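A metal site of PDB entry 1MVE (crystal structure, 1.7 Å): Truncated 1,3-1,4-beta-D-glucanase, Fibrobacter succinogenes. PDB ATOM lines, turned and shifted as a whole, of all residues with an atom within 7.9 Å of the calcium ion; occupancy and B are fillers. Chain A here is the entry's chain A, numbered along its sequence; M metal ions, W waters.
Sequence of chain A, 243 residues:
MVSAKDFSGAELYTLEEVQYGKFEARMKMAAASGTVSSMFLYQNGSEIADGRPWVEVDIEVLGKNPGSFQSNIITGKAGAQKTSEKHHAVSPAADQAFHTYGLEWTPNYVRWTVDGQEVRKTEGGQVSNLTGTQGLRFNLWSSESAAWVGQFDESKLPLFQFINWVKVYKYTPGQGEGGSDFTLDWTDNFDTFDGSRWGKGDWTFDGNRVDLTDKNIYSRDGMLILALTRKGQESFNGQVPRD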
ATOM      1  N   ARG A  26     -27.337 -24.050 -18.330  1.00  0.00           N
ATOM      2  CA  ARG A  26     -27.055 -23.664 -16.959  1.00  0.00           C
ATOM      3  C   ARG A  26     -27.577 -22.228 -16.803  1.00  0.00           C
ATOM      4  O   ARG A  26     -27.015 -21.307 -17.390  1.00  0.00           O
ATOM      5  CB  ARG A  26     -25.550 -23.676 -16.757  1.00  0.00           C
ATOM      6  CG  ARG A  26     -25.132 -23.325 -15.363  1.00  0.00           C
ATOM      7  CD  ARG A  26     -25.403 -24.449 -14.389  1.00  0.00           C
ATOM      8  NE  ARG A  26     -25.009 -24.026 -13.059  1.00  0.00           N
ATOM      9  CZ  ARG A  26     -25.286 -24.672 -11.935  1.00  0.00           C
ATOM     10  NH1 ARG A  26     -25.977 -25.813 -11.960  1.00  0.00           N
ATOM     11  NH2 ARG A  26     -24.862 -24.158 -10.777  1.00  0.00           N
ATOM     12  N   ILE A 163     -28.002 -16.870 -18.630  1.00  0.00           N
ATOM     13  CA  ILE A 163     -27.605 -18.159 -19.156  1.00  0.00           C
ATOM     14  C   ILE A 163     -26.078 -18.234 -19.137  1.00  0.00           C
ATOM     15  O   ILE A 163     -25.398 -17.517 -19.872  1.00  0.00           O
ATOM     16  CB  ILE A 163     -28.125 -18.365 -20.598  1.00  0.00           C
ATOM     17  CG1 ILE A 163     -29.623 -18.084 -20.649  1.00  0.00           C
ATOM     18  CG2 ILE A 163     -27.836 -19.789 -21.033  1.00  0.00           C
ATOM     19  CD1 ILE A 163     -30.289 -18.336 -22.010  1.00  0.00           C
ATOM     20  N   ASN A 164     -25.553 -19.090 -18.277  1.00  0.00           N
ATOM     21  CA  ASN A 164     -24.107 -19.268 -18.138  1.00  0.00           C
ATOM     22  C   ASN A 164     -23.499 -20.052 -19.295  1.00  0.00           C
ATOM     23  O   ASN A 164     -22.438 -19.700 -19.821  1.00  0.00           O
ATOM     24  CB  ASN A 164     -23.799 -20.003 -16.826  1.00  0.00           C
ATOM     25  CG  ASN A 164     -22.321 -19.992 -16.484  1.00  0.00           C
ATOM     26  OD1 ASN A 164     -21.518 -19.422 -17.208  1.00  0.00           O
ATOM     27  ND2 ASN A 164     -21.963 -20.612 -15.364  1.00  0.00           N
ATOM     28  N   TRP A 165     -24.146 -21.155 -19.675  1.00  0.00           N
ATOM     29  CA  TRP A 165     -23.690 -21.952 -20.787  1.00  0.00           C
ATOM     30  C   TRP A 165     -24.772 -22.881 -21.284  1.00  0.00           C
ATOM     31  O   TRP A 165     -25.733 -23.179 -20.569  1.00  0.00           O
ATOM     32  CB  TRP A 165     -22.431 -22.798 -20.435  1.00  0.00           C
ATOM     33  CG  TRP A 165     -22.486 -23.665 -19.169  1.00  0.00           C
ATOM     34  CD1 TRP A 165     -21.915 -23.361 -17.966  1.00  0.00           C
ATOM     35  CD2 TRP A 165     -23.118 -24.951 -18.997  1.00  0.00           C
ATOM     36  NE1 TRP A 165     -22.154 -24.376 -17.050  1.00  0.00           N
ATOM     37  CE2 TRP A 165     -22.885 -25.354 -17.663  1.00  0.00           C
ATOM     38  CE3 TRP A 165     -23.858 -25.789 -19.835  1.00  0.00           C
ATOM     39  CZ2 TRP A 165     -23.356 -26.575 -17.138  1.00  0.00           C
ATOM     40  CZ3 TRP A 165     -24.349 -27.007 -19.316  1.00  0.00           C
ATOM     41  CH2 TRP A 165     -24.089 -27.379 -17.987  1.00  0.00           C
ATOM     42  N   VAL A 166     -24.607 -23.331 -22.526  1.00  0.00           N
ATOM     43  CA  VAL A 166     -25.502 -24.270 -23.170  1.00  0.00           C
ATOM     44  C   VAL A 166     -24.678 -25.391 -23.784  1.00  0.00           C
ATOM     45  O   VAL A 166     -23.604 -25.148 -24.335  1.00  0.00           O
ATOM     46  CB  VAL A 166     -26.315 -23.585 -24.279  1.00  0.00           C
ATOM     47  CG1 VAL A 166     -26.825 -24.607 -25.321  1.00  0.00           C
ATOM     48  CG2 VAL A 166     -27.479 -22.888 -23.642  1.00  0.00           C
ATOM     49  N   ASP A 188     -21.660 -23.546 -25.820  1.00  0.00           N
ATOM     50  CA  ASP A 188     -21.502 -22.101 -25.907  1.00  0.00           C
ATOM     51  C   ASP A 188     -21.374 -21.622 -24.464  1.00  0.00           C
ATOM     52  O   ASP A 188     -22.284 -21.851 -23.671  1.00  0.00           O
ATOM     53  CB  ASP A 188     -22.713 -21.433 -26.552  1.00  0.00           C
ATOM     54  CG  ASP A 188     -22.426 -20.017 -26.996  1.00  0.00           C
ATOM     55  OD1 ASP A 188     -21.632 -19.334 -26.313  1.00  0.00           O
ATOM     56  OD2 ASP A 188     -22.982 -19.570 -28.022  1.00  0.00           O
ATOM     57  N   ASN A 189     -20.275 -20.962 -24.122  1.00  0.00           N
ATOM     58  CA  ASN A 189     -20.057 -20.473 -22.767  1.00  0.00           C
ATOM     59  C   ASN A 189     -20.474 -19.006 -22.633  1.00  0.00           C
ATOM     60  O   ASN A 189     -20.321 -18.403 -21.582  1.00  0.00           O
ATOM     61  CB  ASN A 189     -18.591 -20.673 -22.378  1.00  0.00           C
ATOM     62  CG  ASN A 189     -18.287 -22.118 -22.032  1.00  0.00           C
ATOM     63  OD1 ASN A 189     -18.841 -22.678 -21.072  1.00  0.00           O
ATOM     64  ND2 ASN A 189     -17.433 -22.756 -22.841  1.00  0.00           N
ATOM     65  N   PHE A 190     -21.012 -18.470 -23.715  1.00  0.00           N
ATOM     66  CA  PHE A 190     -21.552 -17.111 -23.758  1.00  0.00           C
ATOM     67  C   PHE A 190     -20.636 -15.971 -23.346  1.00  0.00           C
ATOM     68  O   PHE A 190     -21.054 -15.002 -22.685  1.00  0.00           O
ATOM     69  CB  PHE A 190     -22.861 -17.092 -22.951  1.00  0.00           C
ATOM     70  CG  PHE A 190     -23.959 -17.913 -23.597  1.00  0.00           C
ATOM     71  CD1 PHE A 190     -24.481 -19.040 -22.955  1.00  0.00           C
ATOM     72  CD2 PHE A 190     -24.421 -17.589 -24.864  1.00  0.00           C
ATOM     73  CE1 PHE A 190     -25.442 -19.840 -23.594  1.00  0.00           C
ATOM     74  CE2 PHE A 190     -25.381 -18.379 -25.500  1.00  0.00           C
ATOM     75  CZ  PHE A 190     -25.891 -19.505 -24.865  1.00  0.00           C
ATOM     76  N   ASP A 191     -19.366 -16.098 -23.739  1.00  0.00           N
ATOM     77  CA  ASP A 191     -18.414 -15.029 -23.486  1.00  0.00           C
ATOM     78  C   ASP A 191     -18.740 -13.954 -24.526  1.00  0.00           C
ATOM     79  O   ASP A 191     -18.255 -12.835 -24.454  1.00  0.00           O
ATOM     80  CB  ASP A 191     -16.975 -15.531 -23.666  1.00  0.00           C
ATOM     81  CG  ASP A 191     -16.510 -16.382 -22.487  1.00  0.00           C
ATOM     82  OD1 ASP A 191     -17.115 -16.264 -21.413  1.00  0.00           O
ATOM     83  OD2 ASP A 191     -15.546 -17.155 -22.645  1.00  0.00           O
ATOM     84  N   THR A 192     -19.564 -14.330 -25.504  1.00  0.00           N
ATOM     85  CA  THR A 192     -20.011 -13.410 -26.528  1.00  0.00           C
ATOM     86  C   THR A 192     -21.349 -13.907 -27.055  1.00  0.00           C
ATOM     87  O   THR A 192     -21.750 -15.042 -26.767  1.00  0.00           O
ATOM     88  CB  THR A 192     -19.072 -13.336 -27.757  1.00  0.00           C
ATOM     89  OG1 THR A 192     -19.160 -14.555 -28.498  1.00  0.00           O
ATOM     90  CG2 THR A 192     -17.629 -13.072 -27.346  1.00  0.00           C
ATOM     91  N   ARG A 220     -22.246 -10.415 -21.072  1.00  0.00           N
ATOM     92  CA  ARG A 220     -21.340  -9.715 -20.185  1.00  0.00           C
ATOM     93  C   ARG A 220     -20.807 -10.703 -19.162  1.00  0.00           C
ATOM     94  O   ARG A 220     -21.556 -11.511 -18.637  1.00  0.00           O
ATOM     95  CB  ARG A 220     -22.071  -8.592 -19.453  1.00  0.00           C
ATOM     96  CG  ARG A 220     -21.236  -7.934 -18.373  1.00  0.00           C
ATOM     97  CD  ARG A 220     -20.015  -7.250 -18.963  1.00  0.00           C
ATOM     98  NE  ARG A 220     -19.089  -6.773 -17.924  1.00  0.00           N
ATOM     99  CZ  ARG A 220     -18.505  -5.582 -17.941  1.00  0.00           C
ATOM    100  NH1 ARG A 220     -18.742  -4.727 -18.926  1.00  0.00           N
ATOM    101  NH2 ARG A 220     -17.677  -5.249 -16.962  1.00  0.00           N
ATOM    102  N   ASP A 221     -19.503 -10.642 -18.885  1.00  0.00           N
ATOM    103  CA  ASP A 221     -18.895 -11.513 -17.882  1.00  0.00           C
ATOM    104  C   ASP A 221     -19.226 -12.998 -17.982  1.00  0.00           C
ATOM    105  O   ASP A 221     -19.456 -13.660 -16.955  1.00  0.00           O
ATOM    106  CB  ASP A 221     -19.277 -11.013 -16.480  1.00  0.00           C
ATOM    107  CG  ASP A 221     -18.674  -9.662 -16.154  1.00  0.00           C
ATOM    108  OD1 ASP A 221     -17.859  -9.181 -16.964  1.00  0.00           O
ATOM    109  OD2 ASP A 221     -19.016  -9.081 -15.108  1.00  0.00           O
ATOM    110  N   GLY A 222     -19.225 -13.529 -19.202  1.00  0.00           N
ATOM    111  CA  GLY A 222     -19.499 -14.930 -19.423  1.00  0.00           C
ATOM    112  C   GLY A 222     -20.953 -15.354 -19.283  1.00  0.00           C
ATOM    113  O   GLY A 222     -21.240 -16.549 -19.170  1.00  0.00           O
ATOM    114  N   MET A 223     -21.859 -14.396 -19.273  1.00  0.00           N
ATOM    115  CA  MET A 223     -23.271 -14.721 -19.158  1.00  0.00           C
ATOM    116  C   MET A 223     -24.042 -14.111 -20.306  1.00  0.00           C
ATOM    117  O   MET A 223     -23.732 -13.004 -20.729  1.00  0.00           O
ATOM    118  CB  MET A 223     -23.878 -14.120 -17.876  1.00  0.00           C
ATOM    119  CG  MET A 223     -23.319 -14.631 -16.596  1.00  0.00           C
ATOM    120  SD  MET A 223     -24.215 -16.254 -16.145  1.00  0.00           S
ATOM    121  CE  MET A 223     -23.030 -16.820 -14.698  1.00  0.00           C
ATOM    122  N   LEU A 224     -25.039 -14.832 -20.815  1.00  0.00           N
ATOM    123  CA  LEU A 224     -25.910 -14.277 -21.860  1.00  0.00           C
ATOM    124  C   LEU A 224     -27.081 -13.779 -21.007  1.00  0.00           C
ATOM    125  O   LEU A 224     -27.620 -14.527 -20.191  1.00  0.00           O
ATOM    126  CB  LEU A 224     -26.367 -15.376 -22.829  1.00  0.00           C
ATOM    127  CG  LEU A 224     -27.106 -14.976 -24.122  1.00  0.00           C
ATOM    128  CD1 LEU A 224     -28.593 -14.723 -23.863  1.00  0.00           C
ATOM    129  CD2 LEU A 224     -26.408 -13.788 -24.723  1.00  0.00           C
ATOM    130  N   ASP A 243     -21.642 -17.885 -10.866  1.00  0.00           N
ATOM    131  CA  ASP A 243     -22.135 -19.258 -10.782  1.00  0.00           C
ATOM    132  C   ASP A 243     -20.971 -20.154 -10.344  1.00  0.00           C
ATOM    133  O   ASP A 243     -20.602 -20.143  -9.168  1.00  0.00           O
ATOM    134  CB  ASP A 243     -22.653 -19.727 -12.142  1.00  0.00           C
ATOM    135  CG  ASP A 243     -23.203 -21.147 -12.100  1.00  0.00           C
ATOM    136  OD1 ASP A 243     -23.410 -21.729 -13.173  1.00  0.00           O
ATOM    137  OD2 ASP A 243     -23.425 -21.683 -11.004  1.00  0.00           O
HETATM  138 CA    CA M   1     -20.344 -18.694 -19.116  1.00  0.00          CA
HETATM  139  O   HOH W   1     -19.131 -18.116 -17.196  1.00  0.00           O
HETATM  140  O   HOH W   2     -19.502 -21.003 -19.027  1.00  0.00           O
HETATM  141  O   HOH W   3     -18.052 -18.111 -19.864  1.00  0.00           O
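N of Asn 164 lies close to SD of Met 223, 3.8 Å away. The side-chain carboxylate (OD1) of Asp 243 sits at hydrogen-bond distance from the side-chain amide nitrogen (ND2) of Asn 164 (2.9 Å). O of Arg 26 is in hydrogen-bond range of N of Asn 164, at 2.8 Å.
Three residues have an atom within 4 Å of the calcium ion: Asn 164, Asn 189 and Gly 222. The nearest printed residue that does not touch the calcium ion is Met 223 (4.6 Å).
The calcium ion is bound by O of Gly 222, water W1, OD1 of Asn 164, O of Asn 164, water W2, water W3 and O of Asn 189.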
